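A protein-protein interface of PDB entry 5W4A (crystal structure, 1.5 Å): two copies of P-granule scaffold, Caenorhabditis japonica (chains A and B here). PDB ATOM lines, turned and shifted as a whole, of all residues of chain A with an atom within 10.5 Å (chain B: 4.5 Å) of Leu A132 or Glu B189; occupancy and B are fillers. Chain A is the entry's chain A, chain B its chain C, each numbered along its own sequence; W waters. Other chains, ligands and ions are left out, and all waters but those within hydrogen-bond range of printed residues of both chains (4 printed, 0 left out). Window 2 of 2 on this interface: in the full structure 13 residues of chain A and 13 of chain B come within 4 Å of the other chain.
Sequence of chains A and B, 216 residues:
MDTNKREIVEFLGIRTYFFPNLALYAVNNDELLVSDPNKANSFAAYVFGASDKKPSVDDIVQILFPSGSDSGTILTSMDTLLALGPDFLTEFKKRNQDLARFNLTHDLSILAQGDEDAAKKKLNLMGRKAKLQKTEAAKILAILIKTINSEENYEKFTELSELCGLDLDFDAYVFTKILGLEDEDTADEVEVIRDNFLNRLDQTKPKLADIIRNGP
The side-chain carboxylate (OE1) of Glu B189 lies within salt-bridge range of the guanidinium group (NH2) of Arg A128 (2.9 Å).
O of Leu A132 sits at hydrogen-bond distance from ND2 of Asn B196 (3.0 Å).
NZ of Lys A134 is in hydrogen-bond range of O of Cys B164.
Water W4 lies within hydrogen-bond range of the backbone carbonyl oxygen of Leu A132, the side-chain amino group of Lys A134, the backbone carbonyl oxygen of Cys B164 and the side-chain amide nitrogen of Asn B196.
Water W2 lies within hydrogen-bond range of the side-chain carboxylate of Glu B189 (2.7 Å) and the backbone carbonyl oxygen of Leu A125 (2.9 Å).
Water W3 lies within hydrogen-bond range of OE2 of Glu B189 and NE of Arg A128.
Water W1 lies within hydrogen-bond range of the side-chain amino group of Lys A139 (2.9 Å) and the backbone carbonyl oxygen of Cys B164 (2.9 Å).
No position is printed for both chains.
Of the 7 pairs that touch across the chains among the printed residues, none has its exchanged pair printed and touching as well.
Among the printed residues, pairs that only touch across the chains: Leu A132 with Val B192 (3.6 Å), Lys A134 with Asn B196 (3.7 Å), Leu A132 with Glu B189 (3.8 Å) and Leu A132 with Cys B164 (3.97 Å).
SG of Cys B164 sits close to O of Ser B161 (3.5 Å).
The backbone carbonyl oxygen (O) of Val B192 lies close to the side-chain amide oxygen (OD1) of Asn B196, 3.4 Å away.
Leu A132 touches just these residues of chain B: Cys B164, Glu B189, Val B192 and Asn B196.
No residue of chain A comes within 4 Å of Ser B161.
Cys B164 touches just these residues of chain A: Leu A132 (3.97 Å) and Lys A134 (3.0 Å).
No residue of chain A comes within 4 Å of Ala B187.
No residue of chain A comes within 4 Å of Val B190.
No residue of chain A comes within 4 Å of Ile B193.
Printed residues of chain B within 4 Å of Lys A134: Cys B164 (3.0 Å) and Asn B196 (3.7 Å).
Printed residues of chain A within 4 Å of Asn B196: Leu A132 (3.0 Å) and Lys A134 (3.7 Å).
Ala A138 touches none of the printed residues of chain B.
Lys A139 touches none of the printed residues of chain B.
The nearest printed residue of chain A that does not touch Asn B196 is Gln A133 (5.2 Å).
Of the 25 printed residues of chain A, 3 touch a printed residue of chain B.
Printed residues of chain A that touch a printed residue of chain B: Arg A128, Leu A132 and Lys A134.
Hydrophobic or aromatic side chains of chain A within 4 Å of the printed part of chain B: Leu A132.
Of the 12 printed residues of chain B, 4 touch a printed residue of chain A.
Hydrophobic or aromatic side chains of chain B within 4 Å of the printed part of chain A: Val B192.
Among the printed residues, 7 pairs touch across the chains.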
ATOM      1  N   LYS A 121       7.480  -4.623 -42.328  1.00  0.00           N
ATOM      2  CA  LYS A 121       6.328  -3.788 -41.979  1.00  0.00           C
ATOM      3  C   LYS A 121       5.434  -4.473 -40.952  1.00  0.00           C
ATOM      4  O   LYS A 121       4.963  -3.840 -39.997  1.00  0.00           O
ATOM      5  CB  LYS A 121       5.521  -3.451 -43.232  1.00  0.00           C
ATOM      6  CG  LYS A 121       6.297  -2.666 -44.280  1.00  0.00           C
ATOM      7  CD  LYS A 121       6.729  -1.282 -43.775  1.00  0.00           C
ATOM      8  CE  LYS A 121       7.714  -0.618 -44.735  1.00  0.00           C
ATOM      9  NZ  LYS A 121       8.157   0.717 -44.254  1.00  0.00           N
ATOM     10  N   LYS A 122       5.203  -5.774 -41.129  1.00  0.00           N
ATOM     11  CA  LYS A 122       4.434  -6.539 -40.157  1.00  0.00           C
ATOM     12  C   LYS A 122       5.153  -6.588 -38.807  1.00  0.00           C
ATOM     13  O   LYS A 122       4.525  -6.431 -37.745  1.00  0.00           O
ATOM     14  CB  LYS A 122       4.203  -7.950 -40.701  1.00  0.00           C
ATOM     15  CG  LYS A 122       3.555  -8.911 -39.716  1.00  0.00           C
ATOM     16  CD  LYS A 122       3.218 -10.242 -40.399  1.00  0.00           C
ATOM     17  CE  LYS A 122       2.782 -11.305 -39.392  1.00  0.00           C
ATOM     18  NZ  LYS A 122       3.904 -11.711 -38.490  1.00  0.00           N
ATOM     19  N   LEU A 123       6.471  -6.824 -38.834  1.00  0.00           N
ATOM     20  CA  LEU A 123       7.224  -6.871 -37.588  1.00  0.00           C
ATOM     21  C   LEU A 123       7.249  -5.507 -36.913  1.00  0.00           C
ATOM     22  O   LEU A 123       7.170  -5.445 -35.682  1.00  0.00           O
ATOM     23  CB  LEU A 123       8.642  -7.389 -37.824  1.00  0.00           C
ATOM     24  CG  LEU A 123       8.741  -8.910 -38.039  1.00  0.00           C
ATOM     25  CD1 LEU A 123      10.171  -9.318 -38.291  1.00  0.00           C
ATOM     26  CD2 LEU A 123       8.166  -9.714 -36.880  1.00  0.00           C
ATOM     27  N   ASN A 124       7.289  -4.424 -37.689  1.00  0.00           N
ATOM     28  CA  ASN A 124       7.257  -3.087 -37.090  1.00  0.00           C
ATOM     29  C   ASN A 124       6.017  -2.920 -36.209  1.00  0.00           C
ATOM     30  O   ASN A 124       6.109  -2.478 -35.058  1.00  0.00           O
ATOM     31  CB  ASN A 124       7.294  -2.028 -38.182  1.00  0.00           C
ATOM     32  CG  ASN A 124       7.107  -0.622 -37.629  1.00  0.00           C
ATOM     33  OD1 ASN A 124       7.894  -0.168 -36.787  1.00  0.00           O
ATOM     34  ND2 ASN A 124       6.095   0.083 -38.114  1.00  0.00           N
ATOM     35  N   LEU A 125       4.851  -3.306 -36.719  1.00  0.00           N
ATOM     36  CA  LEU A 125       3.641  -3.150 -35.924  1.00  0.00           C
ATOM     37  C   LEU A 125       3.661  -4.071 -34.719  1.00  0.00           C
ATOM     38  O   LEU A 125       3.239  -3.671 -33.623  1.00  0.00           O
ATOM     39  CB  LEU A 125       2.402  -3.416 -36.783  1.00  0.00           C
ATOM     40  CG  LEU A 125       2.237  -2.477 -37.961  1.00  0.00           C
ATOM     41  CD1 LEU A 125       0.917  -2.787 -38.681  1.00  0.00           C
ATOM     42  CD2 LEU A 125       2.297  -0.992 -37.595  1.00  0.00           C
ATOM     43  N   MET A 126       4.176  -5.300 -34.873  1.00  0.00           N
ATOM     44  CA  MET A 126       4.251  -6.181 -33.728  1.00  0.00           C
ATOM     45  C   MET A 126       5.202  -5.648 -32.660  1.00  0.00           C
ATOM     46  O   MET A 126       4.902  -5.768 -31.455  1.00  0.00           O
ATOM     47  CB  MET A 126       4.656  -7.578 -34.161  1.00  0.00           C
ATOM     48  CG  MET A 126       3.621  -8.177 -35.061  1.00  0.00           C
ATOM     49  SD  MET A 126       4.200  -9.881 -35.720  1.00  0.00           S
ATOM     50  CE  MET A 126       4.496 -10.704 -33.968  1.00  0.00           C
ATOM     51  N   GLY A 127       6.314  -5.039 -33.078  1.00  0.00           N
ATOM     52  CA  GLY A 127       7.258  -4.509 -32.108  1.00  0.00           C
ATOM     53  C   GLY A 127       6.678  -3.355 -31.316  1.00  0.00           C
ATOM     54  O   GLY A 127       6.954  -3.210 -30.133  1.00  0.00           O
ATOM     55  N   ARG A 128       5.899  -2.503 -31.975  1.00  0.00           N
ATOM     56  CA  ARG A 128       5.294  -1.374 -31.288  1.00  0.00           C
ATOM     57  C   ARG A 128       4.323  -1.850 -30.222  1.00  0.00           C
ATOM     58  O   ARG A 128       4.261  -1.273 -29.140  1.00  0.00           O
ATOM     59  CB  ARG A 128       4.606  -0.463 -32.309  1.00  0.00           C
ATOM     60  CG  ARG A 128       5.579   0.231 -33.312  1.00  0.00           C
ATOM     61  CD  ARG A 128       4.858   0.998 -34.388  1.00  0.00           C
ATOM     62  NE  ARG A 128       4.068   2.077 -33.797  1.00  0.00           N
ATOM     63  CZ  ARG A 128       4.465   3.333 -33.674  1.00  0.00           C
ATOM     64  NH1 ARG A 128       5.658   3.729 -34.125  1.00  0.00           N
ATOM     65  NH2 ARG A 128       3.648   4.207 -33.095  1.00  0.00           N
ATOM     66  N   LYS A 129       3.562  -2.914 -30.509  1.00  0.00           N
ATOM     67  CA  LYS A 129       2.646  -3.448 -29.504  1.00  0.00           C
ATOM     68  C   LYS A 129       3.397  -4.179 -28.401  1.00  0.00           C
ATOM     69  O   LYS A 129       3.008  -4.110 -27.220  1.00  0.00           O
ATOM     70  CB  LYS A 129       1.601  -4.362 -30.150  1.00  0.00           C
ATOM     71  CG  LYS A 129       0.589  -3.566 -30.955  1.00  0.00           C
ATOM     72  CD  LYS A 129      -0.572  -4.443 -31.430  1.00  0.00           C
ATOM     73  CE  LYS A 129      -0.274  -5.077 -32.775  1.00  0.00           C
ATOM     74  NZ  LYS A 129      -1.479  -5.748 -33.355  1.00  0.00           N
ATOM     75  N   ALA A 130       4.474  -4.882 -28.764  1.00  0.00           N
ATOM     76  CA  ALA A 130       5.261  -5.602 -27.771  1.00  0.00           C
ATOM     77  C   ALA A 130       5.863  -4.661 -26.736  1.00  0.00           C
ATOM     78  O   ALA A 130       5.899  -4.985 -25.545  1.00  0.00           O
ATOM     79  CB  ALA A 130       6.366  -6.428 -28.451  1.00  0.00           C
ATOM     80  N   LYS A 131       6.316  -3.484 -27.159  1.00  0.00           N
ATOM     81  CA  LYS A 131       6.989  -2.557 -26.265  1.00  0.00           C
ATOM     82  C   LYS A 131       6.044  -2.065 -25.172  1.00  0.00           C
ATOM     83  O   LYS A 131       6.481  -1.799 -24.049  1.00  0.00           O
ATOM     84  CB  LYS A 131       7.551  -1.377 -27.042  1.00  0.00           C
ATOM     85  CG  LYS A 131       8.407  -0.480 -26.209  1.00  0.00           C
ATOM     86  CD  LYS A 131       9.244   0.478 -27.070  1.00  0.00           C
ATOM     87  CE  LYS A 131      10.233   1.261 -26.201  1.00  0.00           C
ATOM     88  NZ  LYS A 131      11.063   2.200 -27.034  1.00  0.00           N
ATOM     89  N   LEU A 132       4.747  -2.024 -25.482  1.00  0.00           N
ATOM     90  CA  LEU A 132       3.720  -1.591 -24.535  1.00  0.00           C
ATOM     91  C   LEU A 132       3.358  -2.639 -23.510  1.00  0.00           C
ATOM     92  O   LEU A 132       2.607  -2.323 -22.564  1.00  0.00           O
ATOM     93  CB  LEU A 132       2.483  -1.180 -25.317  1.00  0.00           C
ATOM     94  CG  LEU A 132       2.669   0.031 -26.246  1.00  0.00           C
ATOM     95  CD1 LEU A 132       1.418   0.228 -27.153  1.00  0.00           C
ATOM     96  CD2 LEU A 132       3.029   1.323 -25.517  1.00  0.00           C
ATOM     97  N   GLN A 133       3.837  -3.874 -23.663  1.00  0.00           N
ATOM     98  CA  GLN A 133       3.650  -4.900 -22.655  1.00  0.00           C
ATOM     99  C   GLN A 133       4.600  -4.632 -21.501  1.00  0.00           C
ATOM    100  O   GLN A 133       5.557  -3.863 -21.608  1.00  0.00           O
ATOM    101  CB  GLN A 133       3.869  -6.295 -23.261  1.00  0.00           C
ATOM    102  CG  GLN A 133       2.855  -6.616 -24.324  1.00  0.00           C
ATOM    103  CD  GLN A 133       3.050  -7.971 -24.962  1.00  0.00           C
ATOM    104  OE1 GLN A 133       3.571  -8.904 -24.345  1.00  0.00           O
ATOM    105  NE2 GLN A 133       2.625  -8.086 -26.213  1.00  0.00           N
ATOM    106  N   LYS A 134       4.280  -5.208 -20.350  1.00  0.00           N
ATOM    107  CA  LYS A 134       5.000  -4.863 -19.137  1.00  0.00           C
ATOM    108  C   LYS A 134       6.128  -5.817 -18.767  1.00  0.00           C
ATOM    109  O   LYS A 134       6.747  -5.644 -17.701  1.00  0.00           O
ATOM    110  CB  LYS A 134       4.018  -4.773 -17.974  1.00  0.00           C
ATOM    111  CG  LYS A 134       2.893  -3.764 -18.180  1.00  0.00           C
ATOM    112  CD  LYS A 134       3.427  -2.403 -18.229  1.00  0.00           C
ATOM    113  CE  LYS A 134       2.318  -1.297 -18.112  1.00  0.00           C
ATOM    114  NZ  LYS A 134       3.045  -0.029 -18.348  1.00  0.00           N
ATOM    115  N   THR A 135       6.481  -6.733 -19.630  1.00  0.00           N
ATOM    116  CA  THR A 135       7.527  -7.704 -19.349  1.00  0.00           C
ATOM    117  C   THR A 135       8.839  -7.372 -20.028  1.00  0.00           C
ATOM    118  O   THR A 135       8.878  -6.780 -21.107  1.00  0.00           O
ATOM    119  CB  THR A 135       7.115  -9.087 -19.827  1.00  0.00           C
ATOM    120  OG1 THR A 135       7.021  -9.107 -21.261  1.00  0.00           O
ATOM    121  CG2 THR A 135       5.749  -9.472 -19.232  1.00  0.00           C
ATOM    122  N   GLU A 136       9.918  -7.826 -19.408  1.00  0.00           N
ATOM    123  CA  GLU A 136      11.238  -7.703 -20.031  1.00  0.00           C
ATOM    124  C   GLU A 136      11.280  -8.454 -21.344  1.00  0.00           C
ATOM    125  O   GLU A 136      11.875  -7.979 -22.316  1.00  0.00           O
ATOM    126  CB  GLU A 136      12.333  -8.219 -19.094  1.00  0.00           C
ATOM    127  CG  GLU A 136      12.546  -7.272 -17.892  1.00  0.00           C
ATOM    128  CD  GLU A 136      13.659  -7.682 -16.954  1.00  0.00           C
ATOM    129  OE1 GLU A 136      13.929  -8.888 -16.841  1.00  0.00           O
ATOM    130  OE2 GLU A 136      14.211  -6.762 -16.310  1.00  0.00           O
ATOM    131  N   ALA A 137      10.674  -9.641 -21.395  1.00  0.00           N
ATOM    132  CA  ALA A 137      10.735 -10.426 -22.617  1.00  0.00           C
ATOM    133  C   ALA A 137      10.119  -9.688 -23.798  1.00  0.00           C
ATOM    134  O   ALA A 137      10.666  -9.722 -24.912  1.00  0.00           O
ATOM    135  CB  ALA A 137      10.046 -11.771 -22.423  1.00  0.00           C
ATOM    136  N   ALA A 138       8.982  -9.032 -23.598  1.00  0.00           N
ATOM    137  CA  ALA A 138       8.359  -8.312 -24.703  1.00  0.00           C
ATOM    138  C   ALA A 138       9.177  -7.090 -25.107  1.00  0.00           C
ATOM    139  O   ALA A 138       9.247  -6.759 -26.298  1.00  0.00           O
ATOM    140  CB  ALA A 138       6.940  -7.884 -24.313  1.00  0.00           C
ATOM    141  N   LYS A 139       9.770  -6.401 -24.131  1.00  0.00           N
ATOM    142  CA  LYS A 139      10.550  -5.196 -24.417  1.00  0.00           C
ATOM    143  C   LYS A 139      11.840  -5.538 -25.168  1.00  0.00           C
ATOM    144  O   LYS A 139      12.252  -4.797 -26.068  1.00  0.00           O
ATOM    145  CB  LYS A 139      10.820  -4.437 -23.114  1.00  0.00           C
ATOM    146  CG  LYS A 139       9.524  -3.832 -22.514  1.00  0.00           C
ATOM    147  CD  LYS A 139       9.743  -3.356 -21.106  1.00  0.00           C
ATOM    148  CE  LYS A 139       8.438  -2.979 -20.425  1.00  0.00           C
ATOM    149  NZ  LYS A 139       7.687  -1.972 -21.220  1.00  0.00           N
ATOM    150  N   ILE A 140      12.428  -6.700 -24.880  1.00  0.00           N
ATOM    151  CA  ILE A 140      13.600  -7.133 -25.632  1.00  0.00           C
ATOM    152  C   ILE A 140      13.219  -7.417 -27.077  1.00  0.00           C
ATOM    153  O   ILE A 140      13.921  -7.011 -28.012  1.00  0.00           O
ATOM    154  CB  ILE A 140      14.254  -8.364 -24.976  1.00  0.00           C
ATOM    155  CG1 ILE A 140      14.834  -8.013 -23.605  1.00  0.00           C
ATOM    156  CG2 ILE A 140      15.356  -8.970 -25.923  1.00  0.00           C
ATOM    157  CD1 ILE A 140      15.156  -9.231 -22.792  1.00  0.00           C
ATOM    158  N   LEU A 141      12.111  -8.119 -27.278  1.00  0.00           N
ATOM    159  CA  LEU A 141      11.619  -8.383 -28.622  1.00  0.00           C
ATOM    160  C   LEU A 141      11.404  -7.082 -29.398  1.00  0.00           C
ATOM    161  O   LEU A 141      11.776  -6.975 -30.579  1.00  0.00           O
ATOM    162  CB  LEU A 141      10.323  -9.189 -28.549  1.00  0.00           C
ATOM    163  CG  LEU A 141       9.601  -9.427 -29.874  1.00  0.00           C
ATOM    164  CD1 LEU A 141      10.454 -10.122 -30.899  1.00  0.00           C
ATOM    165  CD2 LEU A 141       8.261 -10.186 -29.602  1.00  0.00           C
ATOM    166  N   ALA A 142      10.799  -6.085 -28.750  1.00  0.00           N
ATOM    167  CA  ALA A 142      10.557  -4.806 -29.418  1.00  0.00           C
ATOM    168  C   ALA A 142      11.861  -4.132 -29.846  1.00  0.00           C
ATOM    169  O   ALA A 142      11.974  -3.644 -30.981  1.00  0.00           O
ATOM    170  CB  ALA A 142       9.744  -3.901 -28.490  1.00  0.00           C
ATOM    171  N   ILE A 143      12.866  -4.106 -28.962  1.00  0.00           N
ATOM    172  CA  ILE A 143      14.160  -3.514 -29.300  1.00  0.00           C
ATOM    173  C   ILE A 143      14.817  -4.278 -30.437  1.00  0.00           C
ATOM    174  O   ILE A 143      15.377  -3.688 -31.364  1.00  0.00           O
ATOM    175  CB  ILE A 143      15.063  -3.475 -28.061  1.00  0.00           C
ATOM    176  CG1 ILE A 143      14.518  -2.470 -27.054  1.00  0.00           C
ATOM    177  CG2 ILE A 143      16.515  -3.115 -28.459  1.00  0.00           C
ATOM    178  CD1 ILE A 143      15.029  -2.651 -25.637  1.00  0.00           C
ATOM    179  N   LYS A 146      13.099  -3.327 -33.672  1.00  0.00           N
ATOM    180  CA  LYS A 146      13.427  -1.970 -34.088  1.00  0.00           C
ATOM    181  C   LYS A 146      14.849  -1.868 -34.612  1.00  0.00           C
ATOM    182  O   LYS A 146      15.113  -1.097 -35.536  1.00  0.00           O
ATOM    183  CB  LYS A 146      13.194  -1.003 -32.935  1.00  0.00           C
ATOM    184  CG  LYS A 146      11.695  -0.852 -32.640  1.00  0.00           C
ATOM    185  CD  LYS A 146      11.461  -0.073 -31.364  1.00  0.00           C
ATOM    186  CE  LYS A 146       9.974  -0.057 -30.969  1.00  0.00           C
ATOM    187  NZ  LYS A 146       9.161   0.579 -32.034  1.00  0.00           N
ATOM    188  N   LEU A 166      16.544  -1.252 -19.810  1.00  0.00           N
ATOM    189  CA  LEU A 166      16.443  -2.538 -19.126  1.00  0.00           C
ATOM    190  C   LEU A 166      17.715  -2.868 -18.365  1.00  0.00           C
ATOM    191  O   LEU A 166      17.921  -4.025 -17.981  1.00  0.00           O
ATOM    192  CB  LEU A 166      16.161  -3.640 -20.144  1.00  0.00           C
ATOM    193  CG  LEU A 166      14.938  -3.454 -21.058  1.00  0.00           C
ATOM    194  CD1 LEU A 166      14.849  -4.518 -22.156  1.00  0.00           C
ATOM    195  CD2 LEU A 166      13.682  -3.445 -20.219  1.00  0.00           C
ATOM    196  N   PHE B 157       2.632  10.740 -30.949  1.00  0.00           N
ATOM    197  CA  PHE B 157       2.079   9.560 -30.280  1.00  0.00           C
ATOM    198  C   PHE B 157       3.161   8.523 -29.975  1.00  0.00           C
ATOM    199  O   PHE B 157       3.209   7.964 -28.870  1.00  0.00           O
ATOM    200  CB  PHE B 157       0.972   8.935 -31.131  1.00  0.00           C
ATOM    201  CG  PHE B 157       0.438   7.679 -30.542  1.00  0.00           C
ATOM    202  CD1 PHE B 157      -0.366   7.732 -29.414  1.00  0.00           C
ATOM    203  CD2 PHE B 157       0.761   6.440 -31.067  1.00  0.00           C
ATOM    204  CE1 PHE B 157      -0.841   6.587 -28.842  1.00  0.00           C
ATOM    205  CE2 PHE B 157       0.263   5.291 -30.500  1.00  0.00           C
ATOM    206  CZ  PHE B 157      -0.532   5.372 -29.378  1.00  0.00           C
ATOM    207  N   SER B 161       4.152   7.523 -26.192  1.00  0.00           N
ATOM    208  CA  SER B 161       3.961   6.130 -25.811  1.00  0.00           C
ATOM    209  C   SER B 161       5.081   5.644 -24.899  1.00  0.00           C
ATOM    210  O   SER B 161       4.868   4.717 -24.113  1.00  0.00           O
ATOM    211  CB  SER B 161       3.895   5.237 -27.054  1.00  0.00           C
ATOM    212  OG  SER B 161       2.655   5.392 -27.761  1.00  0.00           O
ATOM    213  N   CYS B 164       4.598   4.820 -21.163  1.00  0.00           N
ATOM    214  CA  CYS B 164       4.171   3.519 -20.682  1.00  0.00           C
ATOM    215  C   CYS B 164       5.341   2.722 -20.119  1.00  0.00           C
ATOM    216  O   CYS B 164       5.125   1.879 -19.257  1.00  0.00           O
ATOM    217  CB  CYS B 164       3.482   2.743 -21.795  1.00  0.00           C
ATOM    218  SG  CYS B 164       2.004   3.606 -22.438  1.00  0.00           S
ATOM    219  N   THR B 186      -3.115   4.305 -35.227  1.00  0.00           N
ATOM    220  CA  THR B 186      -2.671   4.166 -33.839  1.00  0.00           C
ATOM    221  C   THR B 186      -3.670   3.411 -32.979  1.00  0.00           C
ATOM    222  O   THR B 186      -3.377   3.139 -31.814  1.00  0.00           O
ATOM    223  CB  THR B 186      -2.439   5.545 -33.217  1.00  0.00           C
ATOM    224  OG1 THR B 186      -3.692   6.243 -33.194  1.00  0.00           O
ATOM    225  CG2 THR B 186      -1.379   6.367 -33.984  1.00  0.00           C
ATOM    226  N   ALA B 187      -4.844   3.067 -33.520  1.00  0.00           N
ATOM    227  CA  ALA B 187      -5.940   2.569 -32.682  1.00  0.00           C
ATOM    228  C   ALA B 187      -5.574   1.321 -31.880  1.00  0.00           C
ATOM    229  O   ALA B 187      -5.924   1.207 -30.691  1.00  0.00           O
ATOM    230  CB  ALA B 187      -7.161   2.298 -33.559  1.00  0.00           C
ATOM    231  N   ASP B 188      -4.892   0.353 -32.495  1.00  0.00           N
ATOM    232  CA  ASP B 188      -4.574  -0.867 -31.764  1.00  0.00           C
ATOM    233  C   ASP B 188      -3.616  -0.582 -30.602  1.00  0.00           C
ATOM    234  O   ASP B 188      -3.735  -1.186 -29.530  1.00  0.00           O
ATOM    235  CB  ASP B 188      -3.990  -1.908 -32.722  1.00  0.00           C
ATOM    236  CG  ASP B 188      -5.048  -2.495 -33.658  1.00  0.00           C
ATOM    237  OD1 ASP B 188      -6.235  -2.125 -33.531  1.00  0.00           O
ATOM    238  OD2 ASP B 188      -4.678  -3.310 -34.518  1.00  0.00           O
ATOM    239  N   GLU B 189      -2.675   0.337 -30.795  1.00  0.00           N
ATOM    240  CA  GLU B 189      -1.763   0.688 -29.719  1.00  0.00           C
ATOM    241  C   GLU B 189      -2.469   1.480 -28.623  1.00  0.00           C
ATOM    242  O   GLU B 189      -2.192   1.276 -27.436  1.00  0.00           O
ATOM    243  CB  GLU B 189      -0.583   1.481 -30.275  1.00  0.00           C
ATOM    244  CG  GLU B 189       0.324   0.615 -31.157  1.00  0.00           C
ATOM    245  CD  GLU B 189       1.188   1.394 -32.121  1.00  0.00           C
ATOM    246  OE1 GLU B 189       1.628   2.522 -31.803  1.00  0.00           O
ATOM    247  OE2 GLU B 189       1.430   0.872 -33.256  1.00  0.00           O
ATOM    248  N   VAL B 190      -3.367   2.396 -29.010  1.00  0.00           N
ATOM    249  CA  VAL B 190      -4.153   3.130 -28.018  1.00  0.00           C
ATOM    250  C   VAL B 190      -4.942   2.158 -27.155  1.00  0.00           C
ATOM    251  O   VAL B 190      -5.021   2.311 -25.930  1.00  0.00           O
ATOM    252  CB  VAL B 190      -5.074   4.147 -28.697  1.00  0.00           C
ATOM    253  CG1 VAL B 190      -6.027   4.823 -27.667  1.00  0.00           C
ATOM    254  CG2 VAL B 190      -4.265   5.211 -29.432  1.00  0.00           C
ATOM    255  N   GLU B 191      -5.483   1.098 -27.773  1.00  0.00           N
ATOM    256  CA  GLU B 191      -6.223   0.105 -26.996  1.00  0.00           C
ATOM    257  C   GLU B 191      -5.344  -0.581 -25.952  1.00  0.00           C
ATOM    258  O   GLU B 191      -5.787  -0.816 -24.826  1.00  0.00           O
ATOM    259  CB  GLU B 191      -6.882  -0.921 -27.926  1.00  0.00           C
ATOM    260  CG  GLU B 191      -7.708  -1.915 -27.153  1.00  0.00           C
ATOM    261  CD  GLU B 191      -8.372  -2.963 -28.026  1.00  0.00           C
ATOM    262  OE1 GLU B 191      -7.771  -3.385 -29.041  1.00  0.00           O
ATOM    263  OE2 GLU B 191      -9.499  -3.369 -27.673  1.00  0.00           O
ATOM    264  N   VAL B 192      -4.084  -0.900 -26.288  1.00  0.00           N
ATOM    265  CA  VAL B 192      -3.181  -1.485 -25.311  1.00  0.00           C
ATOM    266  C   VAL B 192      -2.912  -0.505 -24.153  1.00  0.00           C
ATOM    267  O   VAL B 192      -2.906  -0.891 -22.974  1.00  0.00           O
ATOM    268  CB  VAL B 192      -1.869  -1.937 -25.986  1.00  0.00           C
ATOM    269  CG1 VAL B 192      -0.886  -2.432 -24.929  1.00  0.00           C
ATOM    270  CG2 VAL B 192      -2.150  -2.996 -27.046  1.00  0.00           C
ATOM    271  N   ILE B 193      -2.651   0.769 -24.471  1.00  0.00           N
ATOM    272  CA  ILE B 193      -2.409   1.781 -23.449  1.00  0.00           C
ATOM    273  C   ILE B 193      -3.622   1.907 -22.537  1.00  0.00           C
ATOM    274  O   ILE B 193      -3.489   1.939 -21.309  1.00  0.00           O
ATOM    275  CB  ILE B 193      -2.063   3.136 -24.089  1.00  0.00           C
ATOM    276  CG1 ILE B 193      -0.749   3.026 -24.858  1.00  0.00           C
ATOM    277  CG2 ILE B 193      -1.947   4.239 -23.026  1.00  0.00           C
ATOM    278  CD1 ILE B 193      -0.362   4.269 -25.633  1.00  0.00           C
ATOM    279  N   ASN B 196      -3.800  -1.116 -20.289  1.00  0.00           N
ATOM    280  CA  ASN B 196      -2.821  -1.016 -19.205  1.00  0.00           C
ATOM    281  C   ASN B 196      -3.340  -0.135 -18.067  1.00  0.00           C
ATOM    282  O   ASN B 196      -3.216  -0.479 -16.890  1.00  0.00           O
ATOM    283  CB  ASN B 196      -1.498  -0.442 -19.708  1.00  0.00           C
ATOM    284  CG  ASN B 196      -0.735  -1.410 -20.582  1.00  0.00           C
ATOM    285  OD1 ASN B 196      -1.075  -2.607 -20.715  1.00  0.00           O
ATOM    286  ND2 ASN B 196       0.324  -0.884 -21.203  1.00  0.00           N
HETATM  287  O   HOH W   1       6.451  -0.736 -18.962  1.00  0.00           O
HETATM  288  O   HOH W   2       1.078  -1.739 -33.874  1.00  0.00           O
HETATM  289  O   HOH W   3       1.174   2.119 -35.655  1.00  0.00           O
HETATM  290  O   HOH W   4       3.788  -0.472 -20.989  1.00  0.00           O
